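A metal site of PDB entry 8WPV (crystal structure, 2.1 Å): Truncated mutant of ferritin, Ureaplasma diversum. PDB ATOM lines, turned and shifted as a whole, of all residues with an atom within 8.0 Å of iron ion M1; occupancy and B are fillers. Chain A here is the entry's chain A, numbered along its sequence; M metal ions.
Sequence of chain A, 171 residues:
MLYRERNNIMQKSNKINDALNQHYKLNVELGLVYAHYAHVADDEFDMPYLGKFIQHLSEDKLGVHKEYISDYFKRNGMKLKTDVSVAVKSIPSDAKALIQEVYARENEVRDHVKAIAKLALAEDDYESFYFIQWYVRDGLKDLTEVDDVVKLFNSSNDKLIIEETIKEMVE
A ring nitrogen (ND1) of His 65 sits close to the side-chain amide oxygen (OD1) of Asn 27, at 3.4 Å. O of His 65 sits at hydrogen-bond distance from OH of Tyr 135 (2.8 Å). The side-chain amino group (NZ) of Lys 61 lies close to the side-chain carboxylate (OD2) of Asp 142 (3.6 Å).
Four residues have an atom within 4 Å of iron ion M1: Asp 60, His 65, Asp 138 and Asp 142.
Iron ion M1 is bound by the side-chain carboxylate (OD2) of Asp 138 (1.9 Å), a ring nitrogen (NE2) of His 65 (2.1 Å), the side-chain carboxylate (OD2) of Asp 60 (2.1 Å) and the side-chain carboxylate (OD2) of Asp 142 (2.2 Å). Iron ion M1 has four donor atoms within binding distance.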
ATOM      1  N   ASN A  27      22.481 -26.888  -4.801  1.00  0.00           N
ATOM      2  CA  ASN A  27      23.808 -26.336  -5.022  1.00  0.00           C
ATOM      3  C   ASN A  27      24.707 -26.530  -3.805  1.00  0.00           C
ATOM      4  O   ASN A  27      25.901 -26.791  -3.939  1.00  0.00           O
ATOM      5  CB  ASN A  27      23.708 -24.856  -5.385  1.00  0.00           C
ATOM      6  CG  ASN A  27      23.502 -24.648  -6.872  1.00  0.00           C
ATOM      7  OD1 ASN A  27      24.420 -24.827  -7.677  1.00  0.00           O
ATOM      8  ND2 ASN A  27      22.286 -24.262  -7.258  1.00  0.00           N
ATOM      9  N   HIS A  56      37.109 -26.178  -8.049  1.00  0.00           N
ATOM     10  CA  HIS A  56      36.565 -24.915  -8.520  1.00  0.00           C
ATOM     11  C   HIS A  56      35.069 -25.012  -8.767  1.00  0.00           C
ATOM     12  O   HIS A  56      34.333 -24.044  -8.538  1.00  0.00           O
ATOM     13  CB  HIS A  56      37.311 -24.467  -9.782  1.00  0.00           C
ATOM     14  CG  HIS A  56      38.612 -23.785  -9.506  1.00  0.00           C
ATOM     15  ND1 HIS A  56      38.916 -22.537  -9.994  1.00  0.00           N
ATOM     16  CD2 HIS A  56      39.678 -24.173  -8.769  1.00  0.00           C
ATOM     17  CE1 HIS A  56      40.124 -22.188  -9.586  1.00  0.00           C
ATOM     18  NE2 HIS A  56      40.612 -23.160  -8.838  1.00  0.00           N
ATOM     19  N   LEU A  57      34.596 -26.171  -9.231  1.00  0.00           N
ATOM     20  CA  LEU A  57      33.159 -26.387  -9.357  1.00  0.00           C
ATOM     21  C   LEU A  57      32.494 -26.361  -7.993  1.00  0.00           C
ATOM     22  O   LEU A  57      31.397 -25.822  -7.828  1.00  0.00           O
ATOM     23  CB  LEU A  57      32.881 -27.711 -10.053  1.00  0.00           C
ATOM     24  CG  LEU A  57      32.591 -27.692 -11.557  1.00  0.00           C
ATOM     25  CD1 LEU A  57      32.365 -29.119 -12.037  1.00  0.00           C
ATOM     26  CD2 LEU A  57      31.371 -26.829 -11.857  1.00  0.00           C
ATOM     27  N   GLU A  59      33.486 -24.718  -5.196  1.00  0.00           N
ATOM     28  CA  GLU A  59      33.376 -23.342  -4.737  1.00  0.00           C
ATOM     29  C   GLU A  59      32.361 -22.562  -5.550  1.00  0.00           C
ATOM     30  O   GLU A  59      31.752 -21.613  -5.054  1.00  0.00           O
ATOM     31  CB  GLU A  59      34.747 -22.659  -4.794  1.00  0.00           C
ATOM     32  CG  GLU A  59      35.701 -23.087  -3.696  1.00  0.00           C
ATOM     33  CD  GLU A  59      37.140 -23.178  -4.166  1.00  0.00           C
ATOM     34  OE1 GLU A  59      37.996 -23.626  -3.375  1.00  0.00           O
ATOM     35  OE2 GLU A  59      37.411 -22.792  -5.321  1.00  0.00           O
ATOM     36  N   ASP A  60      32.157 -22.950  -6.818  1.00  0.00           N
ATOM     37  CA  ASP A  60      31.144 -22.310  -7.644  1.00  0.00           C
ATOM     38  C   ASP A  60      29.748 -22.547  -7.085  1.00  0.00           C
ATOM     39  O   ASP A  60      28.966 -21.607  -6.891  1.00  0.00           O
ATOM     40  CB  ASP A  60      31.254 -22.820  -9.075  1.00  0.00           C
ATOM     41  CG  ASP A  60      30.731 -21.831 -10.093  1.00  0.00           C
ATOM     42  OD1 ASP A  60      30.939 -20.612  -9.910  1.00  0.00           O
ATOM     43  OD2 ASP A  60      30.114 -22.275 -11.086  1.00  0.00           O
ATOM     44  N   LYS A  61      29.409 -23.819  -6.809  1.00  0.00           N
ATOM     45  CA  LYS A  61      28.081 -24.139  -6.295  1.00  0.00           C
ATOM     46  C   LYS A  61      27.886 -23.572  -4.895  1.00  0.00           C
ATOM     47  O   LYS A  61      26.825 -23.009  -4.589  1.00  0.00           O
ATOM     48  CB  LYS A  61      27.882 -25.656  -6.279  1.00  0.00           C
ATOM     49  CG  LYS A  61      28.282 -26.372  -7.565  1.00  0.00           C
ATOM     50  CD  LYS A  61      27.113 -26.529  -8.516  1.00  0.00           C
ATOM     51  CE  LYS A  61      27.561 -26.389  -9.965  1.00  0.00           C
ATOM     52  NZ  LYS A  61      26.421 -26.144 -10.898  1.00  0.00           N
ATOM     53  N   VAL A  64      28.615 -18.376  -5.600  1.00  0.00           N
ATOM     54  CA  VAL A  64      27.631 -17.505  -6.233  1.00  0.00           C
ATOM     55  C   VAL A  64      26.349 -18.263  -6.563  1.00  0.00           C
ATOM     56  O   VAL A  64      25.255 -17.670  -6.554  1.00  0.00           O
ATOM     57  CB  VAL A  64      28.224 -16.833  -7.482  1.00  0.00           C
ATOM     58  CG1 VAL A  64      29.491 -16.077  -7.125  1.00  0.00           C
ATOM     59  CG2 VAL A  64      28.509 -17.870  -8.570  1.00  0.00           C
ATOM     60  N   HIS A  65      26.446 -19.559  -6.859  1.00  0.00           N
ATOM     61  CA  HIS A  65      25.243 -20.316  -7.207  1.00  0.00           C
ATOM     62  C   HIS A  65      24.221 -20.313  -6.089  1.00  0.00           C
ATOM     63  O   HIS A  65      23.012 -20.308  -6.338  1.00  0.00           O
ATOM     64  CB  HIS A  65      25.614 -21.752  -7.578  1.00  0.00           C
ATOM     65  CG  HIS A  65      26.030 -21.927  -9.004  1.00  0.00           C
ATOM     66  ND1 HIS A  65      25.211 -22.480  -9.964  1.00  0.00           N
ATOM     67  CD2 HIS A  65      27.189 -21.605  -9.638  1.00  0.00           C
ATOM     68  CE1 HIS A  65      25.845 -22.501 -11.129  1.00  0.00           C
ATOM     69  NE2 HIS A  65      27.040 -21.973 -10.952  1.00  0.00           N
ATOM     70  N   TYR A  68      23.427 -15.925  -5.002  1.00  0.00           N
ATOM     71  CA  TYR A  68      22.502 -15.228  -5.880  1.00  0.00           C
ATOM     72  C   TYR A  68      21.058 -15.467  -5.459  1.00  0.00           C
ATOM     73  O   TYR A  68      20.227 -14.547  -5.492  1.00  0.00           O
ATOM     74  CB  TYR A  68      22.697 -15.653  -7.338  1.00  0.00           C
ATOM     75  CG  TYR A  68      23.986 -15.226  -7.980  1.00  0.00           C
ATOM     76  CD1 TYR A  68      24.723 -14.163  -7.470  1.00  0.00           C
ATOM     77  CD2 TYR A  68      24.451 -15.861  -9.122  1.00  0.00           C
ATOM     78  CE1 TYR A  68      25.906 -13.766  -8.078  1.00  0.00           C
ATOM     79  CE2 TYR A  68      25.627 -15.472  -9.739  1.00  0.00           C
ATOM     80  CZ  TYR A  68      26.355 -14.421  -9.209  1.00  0.00           C
ATOM     81  OH  TYR A  68      27.523 -14.032  -9.819  1.00  0.00           O
ATOM     82  N   GLU A 106      25.677 -32.571 -13.117  1.00  0.00           N
ATOM     83  CA  GLU A 106      25.540 -31.282 -13.796  1.00  0.00           C
ATOM     84  C   GLU A 106      24.418 -31.321 -14.828  1.00  0.00           C
ATOM     85  O   GLU A 106      23.740 -30.304 -15.033  1.00  0.00           O
ATOM     86  CB  GLU A 106      26.854 -30.885 -14.456  1.00  0.00           C
ATOM     87  CG  GLU A 106      27.937 -30.432 -13.493  1.00  0.00           C
ATOM     88  CD  GLU A 106      27.506 -29.245 -12.647  1.00  0.00           C
ATOM     89  OE1 GLU A 106      27.184 -28.189 -13.232  1.00  0.00           O
ATOM     90  OE2 GLU A 106      27.493 -29.374 -11.407  1.00  0.00           O
ATOM     91  N   VAL A 109      21.203 -30.742 -13.119  1.00  0.00           N
ATOM     92  CA  VAL A 109      21.030 -29.328 -12.787  1.00  0.00           C
ATOM     93  C   VAL A 109      20.306 -28.603 -13.903  1.00  0.00           C
ATOM     94  O   VAL A 109      19.413 -27.777 -13.666  1.00  0.00           O
ATOM     95  CB  VAL A 109      22.388 -28.691 -12.465  1.00  0.00           C
ATOM     96  CG1 VAL A 109      22.294 -27.171 -12.499  1.00  0.00           C
ATOM     97  CG2 VAL A 109      22.894 -29.167 -11.113  1.00  0.00           C
ATOM     98  N   TRP A 134      20.645 -16.450 -15.955  1.00  0.00           N
ATOM     99  CA  TRP A 134      22.037 -16.715 -15.644  1.00  0.00           C
ATOM    100  C   TRP A 134      22.256 -18.187 -15.447  1.00  0.00           C
ATOM    101  O   TRP A 134      23.158 -18.749 -16.009  1.00  0.00           O
ATOM    102  CB  TRP A 134      22.481 -15.958 -14.411  1.00  0.00           C
ATOM    103  CG  TRP A 134      23.931 -16.117 -14.111  1.00  0.00           C
ATOM    104  CD1 TRP A 134      24.951 -15.413 -14.645  1.00  0.00           C
ATOM    105  CD2 TRP A 134      24.519 -17.073 -13.228  1.00  0.00           C
ATOM    106  NE1 TRP A 134      26.142 -15.852 -14.154  1.00  0.00           N
ATOM    107  CE2 TRP A 134      25.899 -16.873 -13.278  1.00  0.00           C
ATOM    108  CE3 TRP A 134      24.008 -18.071 -12.389  1.00  0.00           C
ATOM    109  CZ2 TRP A 134      26.789 -17.637 -12.526  1.00  0.00           C
ATOM    110  CZ3 TRP A 134      24.880 -18.819 -11.657  1.00  0.00           C
ATOM    111  CH2 TRP A 134      26.255 -18.604 -11.726  1.00  0.00           C
ATOM    112  N   TYR A 135      21.408 -18.810 -14.673  1.00  0.00           N
ATOM    113  CA  TYR A 135      21.516 -20.205 -14.404  1.00  0.00           C
ATOM    114  C   TYR A 135      21.311 -21.046 -15.647  1.00  0.00           C
ATOM    115  O   TYR A 135      21.917 -22.060 -15.795  1.00  0.00           O
ATOM    116  CB  TYR A 135      20.526 -20.531 -13.313  1.00  0.00           C
ATOM    117  CG  TYR A 135      20.859 -20.023 -11.950  1.00  0.00           C
ATOM    118  CD1 TYR A 135      20.515 -18.746 -11.566  1.00  0.00           C
ATOM    119  CD2 TYR A 135      21.488 -20.838 -11.022  1.00  0.00           C
ATOM    120  CE1 TYR A 135      20.816 -18.278 -10.310  1.00  0.00           C
ATOM    121  CE2 TYR A 135      21.788 -20.380  -9.769  1.00  0.00           C
ATOM    122  CZ  TYR A 135      21.438 -19.097  -9.420  1.00  0.00           C
ATOM    123  OH  TYR A 135      21.739 -18.627  -8.178  1.00  0.00           O
ATOM    124  N   ARG A 137      22.132 -20.218 -18.710  1.00  0.00           N
ATOM    125  CA  ARG A 137      23.403 -20.165 -19.359  1.00  0.00           C
ATOM    126  C   ARG A 137      24.504 -20.898 -18.600  1.00  0.00           C
ATOM    127  O   ARG A 137      25.196 -21.681 -19.197  1.00  0.00           O
ATOM    128  CB  ARG A 137      23.779 -18.737 -19.624  1.00  0.00           C
ATOM    129  CG  ARG A 137      25.190 -18.476 -20.093  1.00  0.00           C
ATOM    130  CD  ARG A 137      25.270 -17.314 -21.068  1.00  0.00           C
ATOM    131  NE  ARG A 137      26.635 -17.084 -21.558  1.00  0.00           N
ATOM    132  CZ  ARG A 137      26.930 -16.690 -22.790  1.00  0.00           C
ATOM    133  NH1 ARG A 137      25.971 -16.468 -23.676  1.00  0.00           N
ATOM    134  NH2 ARG A 137      28.199 -16.508 -23.147  1.00  0.00           N
ATOM    135  N   ASP A 138      24.650 -20.660 -17.307  1.00  0.00           N
ATOM    136  CA  ASP A 138      25.742 -21.258 -16.557  1.00  0.00           C
ATOM    137  C   ASP A 138      25.593 -22.772 -16.474  1.00  0.00           C
ATOM    138  O   ASP A 138      26.596 -23.487 -16.404  1.00  0.00           O
ATOM    139  CB  ASP A 138      25.826 -20.647 -15.168  1.00  0.00           C
ATOM    140  CG  ASP A 138      27.218 -20.728 -14.594  1.00  0.00           C
ATOM    141  OD1 ASP A 138      28.039 -19.831 -14.870  1.00  0.00           O
ATOM    142  OD2 ASP A 138      27.492 -21.699 -13.855  1.00  0.00           O
ATOM    143  N   GLY A 139      24.358 -23.266 -16.505  1.00  0.00           N
ATOM    144  CA  GLY A 139      24.151 -24.700 -16.556  1.00  0.00           C
ATOM    145  C   GLY A 139      24.756 -25.329 -17.799  1.00  0.00           C
ATOM    146  O   GLY A 139      25.325 -26.421 -17.738  1.00  0.00           O
ATOM    147  N   LEU A 140      24.648 -24.646 -18.946  1.00  0.00           N
ATOM    148  CA  LEU A 140      25.191 -25.206 -20.181  1.00  0.00           C
ATOM    149  C   LEU A 140      26.706 -25.108 -20.219  1.00  0.00           C
ATOM    150  O   LEU A 140      27.361 -25.990 -20.796  1.00  0.00           O
ATOM    151  CB  LEU A 140      24.581 -24.492 -21.394  1.00  0.00           C
ATOM    152  CG  LEU A 140      24.769 -25.244 -22.715  1.00  0.00           C
ATOM    153  CD1 LEU A 140      24.453 -26.717 -22.547  1.00  0.00           C
ATOM    154  CD2 LEU A 140      23.922 -24.624 -23.831  1.00  0.00           C
ATOM    155  N   LYS A 141      27.296 -24.067 -19.632  1.00  0.00           N
ATOM    156  CA  LYS A 141      28.737 -23.892 -19.705  1.00  0.00           C
ATOM    157  C   LYS A 141      29.471 -24.708 -18.666  1.00  0.00           C
ATOM    158  O   LYS A 141      30.547 -25.266 -18.956  1.00  0.00           O
ATOM    159  CB  LYS A 141      29.092 -22.408 -19.583  1.00  0.00           C
ATOM    160  CG  LYS A 141      29.388 -21.781 -20.930  1.00  0.00           C
ATOM    161  CD  LYS A 141      28.201 -21.909 -21.856  1.00  0.00           C
ATOM    162  CE  LYS A 141      27.468 -20.612 -21.972  1.00  0.00           C
ATOM    163  NZ  LYS A 141      26.364 -20.671 -22.956  1.00  0.00           N
ATOM    164  N   ASP A 142      28.927 -24.799 -17.450  1.00  0.00           N
ATOM    165  CA  ASP A 142      29.471 -25.752 -16.482  1.00  0.00           C
ATOM    166  C   ASP A 142      29.456 -27.165 -17.044  1.00  0.00           C
ATOM    167  O   ASP A 142      30.449 -27.896 -16.927  1.00  0.00           O
ATOM    168  CB  ASP A 142      28.684 -25.690 -15.174  1.00  0.00           C
ATOM    169  CG  ASP A 142      29.053 -24.507 -14.310  1.00  0.00           C
ATOM    170  OD1 ASP A 142      30.027 -23.794 -14.658  1.00  0.00           O
ATOM    171  OD2 ASP A 142      28.398 -24.299 -13.268  1.00  0.00           O
ATOM    172  N   LEU A 143      28.348 -27.552 -17.684  1.00  0.00           N
ATOM    173  CA  LEU A 143      28.291 -28.868 -18.304  1.00  0.00           C
ATOM    174  C   LEU A 143      29.267 -28.990 -19.470  1.00  0.00           C
ATOM    175  O   LEU A 143      29.800 -30.080 -19.712  1.00  0.00           O
ATOM    176  CB  LEU A 143      26.863 -29.166 -18.772  1.00  0.00           C
ATOM    177  CG  LEU A 143      26.658 -30.596 -19.244  1.00  0.00           C
ATOM    178  CD1 LEU A 143      26.113 -31.449 -18.120  1.00  0.00           C
ATOM    179  CD2 LEU A 143      25.744 -30.656 -20.463  1.00  0.00           C
ATOM    180  N   GLU A 145      32.228 -27.367 -19.659  1.00  0.00           N
ATOM    181  CA  GLU A 145      33.550 -27.486 -19.043  1.00  0.00           C
ATOM    182  C   GLU A 145      33.792 -28.906 -18.544  1.00  0.00           C
ATOM    183  O   GLU A 145      34.872 -29.475 -18.757  1.00  0.00           O
ATOM    184  CB  GLU A 145      33.688 -26.477 -17.900  1.00  0.00           C
ATOM    185  CG  GLU A 145      33.721 -25.024 -18.340  1.00  0.00           C
ATOM    186  CD  GLU A 145      33.529 -24.072 -17.183  1.00  0.00           C
ATOM    187  OE1 GLU A 145      33.177 -24.532 -16.071  1.00  0.00           O
ATOM    188  OE2 GLU A 145      33.724 -22.854 -17.379  1.00  0.00           O
HETATM  189 FE    FE M   1      28.496 -22.317 -12.368  1.00  0.00          FE
HETATM  190 FE    FE M   2      30.349 -21.053 -14.508  1.00  0.00          FE
HETATM  191 FE    FE M   3      30.642 -19.559 -12.541  1.00  0.00          FE
